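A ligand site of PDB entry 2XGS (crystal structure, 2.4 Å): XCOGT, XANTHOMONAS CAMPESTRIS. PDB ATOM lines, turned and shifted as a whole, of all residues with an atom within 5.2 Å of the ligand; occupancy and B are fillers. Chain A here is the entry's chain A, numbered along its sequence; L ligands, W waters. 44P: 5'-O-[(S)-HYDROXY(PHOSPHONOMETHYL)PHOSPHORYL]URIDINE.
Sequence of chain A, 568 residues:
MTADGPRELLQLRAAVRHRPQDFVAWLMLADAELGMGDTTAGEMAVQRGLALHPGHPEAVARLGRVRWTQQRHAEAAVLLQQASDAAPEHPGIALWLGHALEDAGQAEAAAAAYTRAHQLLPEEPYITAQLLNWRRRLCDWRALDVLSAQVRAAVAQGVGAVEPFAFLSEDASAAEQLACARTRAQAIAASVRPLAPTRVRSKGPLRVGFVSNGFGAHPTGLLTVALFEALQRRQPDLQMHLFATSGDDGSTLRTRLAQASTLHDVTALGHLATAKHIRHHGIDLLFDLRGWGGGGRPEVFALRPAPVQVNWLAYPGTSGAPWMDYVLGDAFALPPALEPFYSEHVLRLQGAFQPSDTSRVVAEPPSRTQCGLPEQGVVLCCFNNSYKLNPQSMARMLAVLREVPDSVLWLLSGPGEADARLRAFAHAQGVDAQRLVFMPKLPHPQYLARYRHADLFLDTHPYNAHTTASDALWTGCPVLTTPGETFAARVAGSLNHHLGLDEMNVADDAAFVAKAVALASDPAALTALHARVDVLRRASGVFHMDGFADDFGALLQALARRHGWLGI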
ATOM      1  N   HIS A 218     -22.674   6.923   2.441  1.00  0.00           N
ATOM      2  CA  HIS A 218     -22.118   8.174   2.927  1.00  0.00           C
ATOM      3  C   HIS A 218     -21.229   8.750   1.824  1.00  0.00           C
ATOM      4  O   HIS A 218     -20.780   8.003   0.967  1.00  0.00           O
ATOM      5  CB  HIS A 218     -21.258   7.881   4.136  1.00  0.00           C
ATOM      6  CG  HIS A 218     -21.996   7.294   5.286  1.00  0.00           C
ATOM      7  ND1 HIS A 218     -22.838   8.033   6.109  1.00  0.00           N
ATOM      8  CD2 HIS A 218     -21.984   6.042   5.802  1.00  0.00           C
ATOM      9  CE1 HIS A 218     -23.309   7.248   7.059  1.00  0.00           C
ATOM     10  NE2 HIS A 218     -22.817   6.035   6.896  1.00  0.00           N
ATOM     11  N   PRO A 219     -20.979  10.075   1.842  1.00  0.00           N
ATOM     12  CA  PRO A 219     -20.116  10.687   0.836  1.00  0.00           C
ATOM     13  C   PRO A 219     -18.873   9.844   0.513  1.00  0.00           C
ATOM     14  O   PRO A 219     -18.638   9.513  -0.650  1.00  0.00           O
ATOM     15  CB  PRO A 219     -19.708  12.028   1.482  1.00  0.00           C
ATOM     16  CG  PRO A 219     -20.857  12.366   2.391  1.00  0.00           C
ATOM     17  CD  PRO A 219     -21.504  11.068   2.814  1.00  0.00           C
ATOM     18  N   LEU A 222     -19.389   6.745  -1.347  1.00  0.00           N
ATOM     19  CA  LEU A 222     -20.017   7.049  -2.590  1.00  0.00           C
ATOM     20  C   LEU A 222     -19.005   7.546  -3.585  1.00  0.00           C
ATOM     21  O   LEU A 222     -19.125   7.273  -4.780  1.00  0.00           O
ATOM     22  CB  LEU A 222     -20.992   8.157  -2.328  1.00  0.00           C
ATOM     23  CG  LEU A 222     -22.236   8.423  -3.125  1.00  0.00           C
ATOM     24  CD1 LEU A 222     -22.781   7.117  -3.718  1.00  0.00           C
ATOM     25  CD2 LEU A 222     -23.254   9.130  -2.129  1.00  0.00           C
ATOM     26  N   ALA A 314     -12.060  14.025   1.734  1.00  0.00           N
ATOM     27  CA  ALA A 314     -13.313  14.459   2.378  1.00  0.00           C
ATOM     28  C   ALA A 314     -13.201  15.449   3.527  1.00  0.00           C
ATOM     29  O   ALA A 314     -14.188  15.739   4.193  1.00  0.00           O
ATOM     30  CB  ALA A 314     -14.244  13.272   2.743  1.00  0.00           C
ATOM     31  N   ASN A 385     -25.878  21.099   2.056  1.00  0.00           N
ATOM     32  CA  ASN A 385     -26.144  21.090   3.510  1.00  0.00           C
ATOM     33  C   ASN A 385     -26.482  22.493   4.070  1.00  0.00           C
ATOM     34  O   ASN A 385     -25.955  23.508   3.588  1.00  0.00           O
ATOM     35  CB  ASN A 385     -24.924  20.514   4.226  1.00  0.00           C
ATOM     36  CG  ASN A 385     -25.181  19.167   4.836  1.00  0.00           C
ATOM     37  OD1 ASN A 385     -25.885  19.065   5.854  1.00  0.00           O
ATOM     38  ND2 ASN A 385     -24.589  18.118   4.254  1.00  0.00           N
ATOM     39  N   TYR A 387     -25.731  24.374   6.730  1.00  0.00           N
ATOM     40  CA  TYR A 387     -24.588  25.203   7.107  1.00  0.00           C
ATOM     41  C   TYR A 387     -23.805  25.791   5.917  1.00  0.00           C
ATOM     42  O   TYR A 387     -22.976  26.688   6.103  1.00  0.00           O
ATOM     43  CB  TYR A 387     -23.658  24.448   8.070  1.00  0.00           C
ATOM     44  CG  TYR A 387     -23.077  23.194   7.507  1.00  0.00           C
ATOM     45  CD1 TYR A 387     -22.009  23.243   6.596  1.00  0.00           C
ATOM     46  CD2 TYR A 387     -23.606  21.943   7.851  1.00  0.00           C
ATOM     47  CE1 TYR A 387     -21.489  22.084   6.048  1.00  0.00           C
ATOM     48  CE2 TYR A 387     -23.087  20.783   7.303  1.00  0.00           C
ATOM     49  CZ  TYR A 387     -22.033  20.849   6.391  1.00  0.00           C
ATOM     50  OH  TYR A 387     -21.534  19.696   5.831  1.00  0.00           O
ATOM     51  N   LYS A 388     -24.044  25.308   4.704  1.00  0.00           N
ATOM     52  CA  LYS A 388     -23.412  25.887   3.505  1.00  0.00           C
ATOM     53  C   LYS A 388     -24.208  27.067   2.952  1.00  0.00           C
ATOM     54  O   LYS A 388     -23.672  27.917   2.214  1.00  0.00           O
ATOM     55  CB  LYS A 388     -23.236  24.830   2.412  1.00  0.00           C
ATOM     56  CG  LYS A 388     -22.367  23.691   2.837  1.00  0.00           C
ATOM     57  CD  LYS A 388     -21.881  22.886   1.640  1.00  0.00           C
ATOM     58  CE  LYS A 388     -21.451  21.508   2.024  1.00  0.00           C
ATOM     59  NZ  LYS A 388     -20.878  20.804   0.830  1.00  0.00           N
ATOM     60  N   LEU A 412     -32.609  21.421  -0.446  1.00  0.00           N
ATOM     61  CA  LEU A 412     -32.706  20.423   0.598  1.00  0.00           C
ATOM     62  C   LEU A 412     -33.436  21.031   1.786  1.00  0.00           C
ATOM     63  O   LEU A 412     -33.058  22.116   2.267  1.00  0.00           O
ATOM     64  CB  LEU A 412     -31.330  20.004   1.082  1.00  0.00           C
ATOM     65  CG  LEU A 412     -30.922  18.575   0.786  1.00  0.00           C
ATOM     66  CD1 LEU A 412     -29.650  18.256   1.570  1.00  0.00           C
ATOM     67  CD2 LEU A 412     -32.059  17.606   1.146  1.00  0.00           C
ATOM     68  N   MET A 439     -36.863  19.834  -0.663  1.00  0.00           N
ATOM     69  CA  MET A 439     -36.790  18.385  -0.819  1.00  0.00           C
ATOM     70  C   MET A 439     -36.477  17.702   0.508  1.00  0.00           C
ATOM     71  O   MET A 439     -35.443  18.013   1.105  1.00  0.00           O
ATOM     72  CB  MET A 439     -35.738  18.004  -1.878  1.00  0.00           C
ATOM     73  CG  MET A 439     -35.698  16.504  -2.156  1.00  0.00           C
ATOM     74  SD  MET A 439     -34.279  15.886  -3.134  1.00  0.00           S
ATOM     75  CE  MET A 439     -32.827  16.437  -2.255  1.00  0.00           C
ATOM     76  N   PRO A 440     -37.345  16.764   0.968  1.00  0.00           N
ATOM     77  CA  PRO A 440     -37.010  15.969   2.135  1.00  0.00           C
ATOM     78  C   PRO A 440     -35.816  15.064   1.837  1.00  0.00           C
ATOM     79  O   PRO A 440     -35.531  14.768   0.675  1.00  0.00           O
ATOM     80  CB  PRO A 440     -38.259  15.108   2.369  1.00  0.00           C
ATOM     81  CG  PRO A 440     -38.846  14.922   1.017  1.00  0.00           C
ATOM     82  CD  PRO A 440     -38.590  16.270   0.330  1.00  0.00           C
ATOM     83  N   LYS A 441     -35.123  14.634   2.879  1.00  0.00           N
ATOM     84  CA  LYS A 441     -33.964  13.791   2.666  1.00  0.00           C
ATOM     85  C   LYS A 441     -34.401  12.485   2.019  1.00  0.00           C
ATOM     86  O   LYS A 441     -35.349  11.835   2.485  1.00  0.00           O
ATOM     87  CB  LYS A 441     -33.268  13.503   3.997  1.00  0.00           C
ATOM     88  CG  LYS A 441     -31.843  12.979   3.871  1.00  0.00           C
ATOM     89  CD  LYS A 441     -31.515  12.363   5.220  1.00  0.00           C
ATOM     90  CE  LYS A 441     -30.365  11.395   5.178  1.00  0.00           C
ATOM     91  NZ  LYS A 441     -30.335  10.297   6.179  1.00  0.00           N
ATOM     92  N   LEU A 442     -33.728  12.085   0.941  1.00  0.00           N
ATOM     93  CA  LEU A 442     -34.113  10.838   0.277  1.00  0.00           C
ATOM     94  C   LEU A 442     -32.957   9.828   0.222  1.00  0.00           C
ATOM     95  O   LEU A 442     -31.810  10.208   0.194  1.00  0.00           O
ATOM     96  CB  LEU A 442     -34.627  11.110  -1.130  1.00  0.00           C
ATOM     97  CG  LEU A 442     -35.919  11.901  -1.221  1.00  0.00           C
ATOM     98  CD1 LEU A 442     -36.039  12.587  -2.547  1.00  0.00           C
ATOM     99  CD2 LEU A 442     -37.193  11.004  -0.855  1.00  0.00           C
ATOM    100  N   PRO A 443     -33.282   8.527   0.184  1.00  0.00           N
ATOM    101  CA  PRO A 443     -32.253   7.565  -0.129  1.00  0.00           C
ATOM    102  C   PRO A 443     -31.546   8.004  -1.394  1.00  0.00           C
ATOM    103  O   PRO A 443     -32.188   8.547  -2.304  1.00  0.00           O
ATOM    104  CB  PRO A 443     -33.046   6.288  -0.383  1.00  0.00           C
ATOM    105  CG  PRO A 443     -34.253   6.447   0.481  1.00  0.00           C
ATOM    106  CD  PRO A 443     -34.606   7.889   0.305  1.00  0.00           C
ATOM    107  N   HIS A 444     -30.235   7.798  -1.437  1.00  0.00           N
ATOM    108  CA  HIS A 444     -29.410   8.328  -2.516  1.00  0.00           C
ATOM    109  C   HIS A 444     -29.946   8.081  -3.936  1.00  0.00           C
ATOM    110  O   HIS A 444     -30.064   9.004  -4.704  1.00  0.00           O
ATOM    111  CB  HIS A 444     -27.969   7.834  -2.353  1.00  0.00           C
ATOM    112  CG  HIS A 444     -27.034   8.371  -3.373  1.00  0.00           C
ATOM    113  ND1 HIS A 444     -26.584   9.677  -3.351  1.00  0.00           N
ATOM    114  CD2 HIS A 444     -26.480   7.791  -4.473  1.00  0.00           C
ATOM    115  CE1 HIS A 444     -25.785   9.867  -4.384  1.00  0.00           C
ATOM    116  NE2 HIS A 444     -25.703   8.744  -5.081  1.00  0.00           N
ATOM    117  N   TYR A 447     -32.890  10.536  -4.448  1.00  0.00           N
ATOM    118  CA  TYR A 447     -32.423  11.922  -4.478  1.00  0.00           C
ATOM    119  C   TYR A 447     -31.698  12.234  -5.783  1.00  0.00           C
ATOM    120  O   TYR A 447     -31.907  13.294  -6.379  1.00  0.00           O
ATOM    121  CB  TYR A 447     -31.539  12.215  -3.229  1.00  0.00           C
ATOM    122  CG  TYR A 447     -30.263  13.019  -3.498  1.00  0.00           C
ATOM    123  CD1 TYR A 447     -30.202  14.376  -3.241  1.00  0.00           C
ATOM    124  CD2 TYR A 447     -29.109  12.393  -4.040  1.00  0.00           C
ATOM    125  CE1 TYR A 447     -29.014  15.114  -3.503  1.00  0.00           C
ATOM    126  CE2 TYR A 447     -27.920  13.097  -4.312  1.00  0.00           C
ATOM    127  CZ  TYR A 447     -27.868  14.452  -4.041  1.00  0.00           C
ATOM    128  OH  TYR A 447     -26.688  15.149  -4.311  1.00  0.00           O
ATOM    129  N   TYR A 463     -18.304  27.750   1.139  1.00  0.00           N
ATOM    130  CA  TYR A 463     -18.201  26.295   1.257  1.00  0.00           C
ATOM    131  C   TYR A 463     -18.990  25.684   0.099  1.00  0.00           C
ATOM    132  O   TYR A 463     -20.203  25.544   0.192  1.00  0.00           O
ATOM    133  CB  TYR A 463     -18.707  25.798   2.648  1.00  0.00           C
ATOM    134  CG  TYR A 463     -18.314  24.372   3.045  1.00  0.00           C
ATOM    135  CD1 TYR A 463     -18.310  23.974   4.380  1.00  0.00           C
ATOM    136  CD2 TYR A 463     -17.943  23.426   2.080  1.00  0.00           C
ATOM    137  CE1 TYR A 463     -17.985  22.690   4.752  1.00  0.00           C
ATOM    138  CE2 TYR A 463     -17.604  22.151   2.426  1.00  0.00           C
ATOM    139  CZ  TYR A 463     -17.624  21.780   3.756  1.00  0.00           C
ATOM    140  OH  TYR A 463     -17.254  20.530   4.096  1.00  0.00           O
ATOM    141  N   ALA A 465     -20.650  23.264  -2.792  1.00  0.00           N
ATOM    142  CA  ALA A 465     -21.125  21.908  -3.027  1.00  0.00           C
ATOM    143  C   ALA A 465     -19.867  21.070  -3.388  1.00  0.00           C
ATOM    144  O   ALA A 465     -19.021  21.536  -4.148  1.00  0.00           O
ATOM    145  CB  ALA A 465     -22.117  21.898  -4.172  1.00  0.00           C
ATOM    146  N   HIS A 466     -19.756  19.886  -2.817  1.00  0.00           N
ATOM    147  CA  HIS A 466     -18.652  18.965  -3.105  1.00  0.00           C
ATOM    148  C   HIS A 466     -19.174  17.659  -3.718  1.00  0.00           C
ATOM    149  O   HIS A 466     -19.155  17.483  -4.933  1.00  0.00           O
ATOM    150  CB  HIS A 466     -17.756  18.732  -1.862  1.00  0.00           C
ATOM    151  CG  HIS A 466     -17.030  19.960  -1.406  1.00  0.00           C
ATOM    152  ND1 HIS A 466     -16.609  20.173  -0.125  1.00  0.00           N
ATOM    153  CD2 HIS A 466     -16.652  21.066  -2.081  1.00  0.00           C
ATOM    154  CE1 HIS A 466     -16.006  21.342  -0.022  1.00  0.00           C
ATOM    155  NE2 HIS A 466     -16.032  21.917  -1.192  1.00  0.00           N
ATOM    156  N   THR A 467     -19.692  16.759  -2.891  1.00  0.00           N
ATOM    157  CA  THR A 467     -20.226  15.497  -3.377  1.00  0.00           C
ATOM    158  C   THR A 467     -21.467  15.791  -4.246  1.00  0.00           C
ATOM    159  O   THR A 467     -21.766  15.131  -5.236  1.00  0.00           O
ATOM    160  CB  THR A 467     -20.647  14.628  -2.181  1.00  0.00           C
ATOM    161  OG1 THR A 467     -19.658  14.711  -1.149  1.00  0.00           O
ATOM    162  CG2 THR A 467     -20.864  13.168  -2.601  1.00  0.00           C
ATOM    163  N   THR A 468     -22.145  16.838  -3.851  1.00  0.00           N
ATOM    164  CA  THR A 468     -23.447  17.185  -4.328  1.00  0.00           C
ATOM    165  C   THR A 468     -23.224  17.773  -5.716  1.00  0.00           C
ATOM    166  O   THR A 468     -24.036  17.565  -6.630  1.00  0.00           O
ATOM    167  CB  THR A 468     -24.047  18.066  -3.200  1.00  0.00           C
ATOM    168  OG1 THR A 468     -25.386  18.472  -3.414  1.00  0.00           O
ATOM    169  CG2 THR A 468     -23.315  19.163  -2.868  1.00  0.00           C
ATOM    170  N   ASP A 471     -22.565  14.886  -7.901  1.00  0.00           N
ATOM    171  CA  ASP A 471     -23.851  14.219  -8.124  1.00  0.00           C
ATOM    172  C   ASP A 471     -24.603  14.898  -9.233  1.00  0.00           C
ATOM    173  O   ASP A 471     -24.947  14.260 -10.222  1.00  0.00           O
ATOM    174  CB  ASP A 471     -24.729  14.282  -6.895  1.00  0.00           C
ATOM    175  CG  ASP A 471     -24.238  13.398  -5.779  1.00  0.00           C
ATOM    176  OD1 ASP A 471     -23.371  12.490  -5.958  1.00  0.00           O
ATOM    177  OD2 ASP A 471     -24.766  13.610  -4.684  1.00  0.00           O
HETATM  178  N1  44P L   1     -27.673  12.981  -0.047  1.00  0.00           N
HETATM  179  C2  44P L   1     -28.637  11.948  -0.359  1.00  0.00           C
HETATM  180  O2  44P L   1     -28.352  10.804  -0.699  1.00  0.00           O
HETATM  181  N3  44P L   1     -30.015  12.228  -0.292  1.00  0.00           N
HETATM  182  C4  44P L   1     -30.499  13.475   0.065  1.00  0.00           C
HETATM  183  O4  44P L   1     -31.729  13.651   0.124  1.00  0.00           O
HETATM  184  C5  44P L   1     -29.587  14.478   0.390  1.00  0.00           C
HETATM  185  C6  44P L   1     -28.203  14.244   0.343  1.00  0.00           C
HETATM  186  PA  44P L   1     -22.393  16.400   2.763  1.00  0.00           P
HETATM  187  PB  44P L   1     -19.815  17.048   1.304  1.00  0.00           P
HETATM  188  C1' 44P L   1     -26.172  12.772  -0.057  1.00  0.00           C
HETATM  189  O1A 44P L   1     -22.422  15.880   4.157  1.00  0.00           O
HETATM  190  O1B 44P L   1     -18.312  16.383   1.542  1.00  0.00           O
HETATM  191  C2' 44P L   1     -25.189  13.100  -1.250  1.00  0.00           C
HETATM  192  O2' 44P L   1     -25.184  12.158  -2.333  1.00  0.00           O
HETATM  193  O2A 44P L   1     -22.644  17.846   2.514  1.00  0.00           O
HETATM  194  O2B 44P L   1     -19.861  18.497   2.092  1.00  0.00           O
HETATM  195  C3' 44P L   1     -23.854  13.057  -0.520  1.00  0.00           C
HETATM  196  O3' 44P L   1     -23.484  11.726  -0.178  1.00  0.00           O
HETATM  197  C3A 44P L   1     -20.896  15.809   2.037  1.00  0.00           C
HETATM  198  O3B 44P L   1     -20.127  17.225  -0.131  1.00  0.00           O
HETATM  199  C4' 44P L   1     -24.167  13.774   0.795  1.00  0.00           C
HETATM  200  O4' 44P L   1     -25.608  13.656   1.018  1.00  0.00           O
HETATM  201  C5' 44P L   1     -23.689  15.221   0.742  1.00  0.00           C
HETATM  202  O5' 44P L   1     -23.600  15.637   2.053  1.00  0.00           O
HETATM  203  O   HOH W   1     -16.842  18.406   2.260  1.00  0.00           O
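Water W1 lies within hydrogen-bond range of O1B of the ligand (2.6 Å), OH of Tyr 463 (2.8 Å) and ND1 of His 466 (3.0 Å).
OH of Tyr 447 lies within hydrogen-bond range of OD2 of Asp 471 (2.5 Å).
The side-chain amide nitrogen (ND2) of Asn 385 sits at hydrogen-bond distance from an oxygen (O2A) of the ligand.
An oxygen (O4) of the ligand lies within hydrogen-bond range of the backbone NH (N) of Leu 442 (2.7 Å).
The backbone carbonyl oxygen (O) of Leu 442 sits at hydrogen-bond distance from a nitrogen (N3) of the ligand, at 2.7 Å.
The backbone NH of Thr 467 sits at hydrogen-bond distance from an oxygen (O3B) of the ligand (2.8 Å).
An oxygen (O3B) of the ligand lies within hydrogen-bond range of the side-chain hydroxyl (OG1) of Thr 467.
The side-chain carboxylate of Asp 471 is in hydrogen-bond range of an oxygen (O2') of the ligand (2.8 Å).
NZ of Lys 388 is in salt-bridge range of O2B of the ligand (2.8 Å).
A ring nitrogen (ND1) of His 444 is in hydrogen-bond range of an oxygen (O2') of the ligand (3.0 Å).
CG of Pro 219 touches C3A of the ligand, at 3.5 Å.
Leu 222 touches the ligand.
Tyr 387 touches the ligand.
Leu 412 touches the ligand.
Met 439 touches the ligand.
CA of Lys 441 touches O4 of the ligand, at 3.4 Å.
CB of Tyr 447 touches N3 of the ligand, at 3.3 Å.
Tyr 463 touches the ligand.
His 466 touches the ligand (CB to O3B, 3.3 Å).
Hydrophobic or aromatic side chains within 4 Å of the ligand: Pro 219, Leu 222, Leu 412, Met 439, His 444, Tyr 447 and His 466.
Of the 21 residues printed, 15 come within 4 Å of the ligand.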
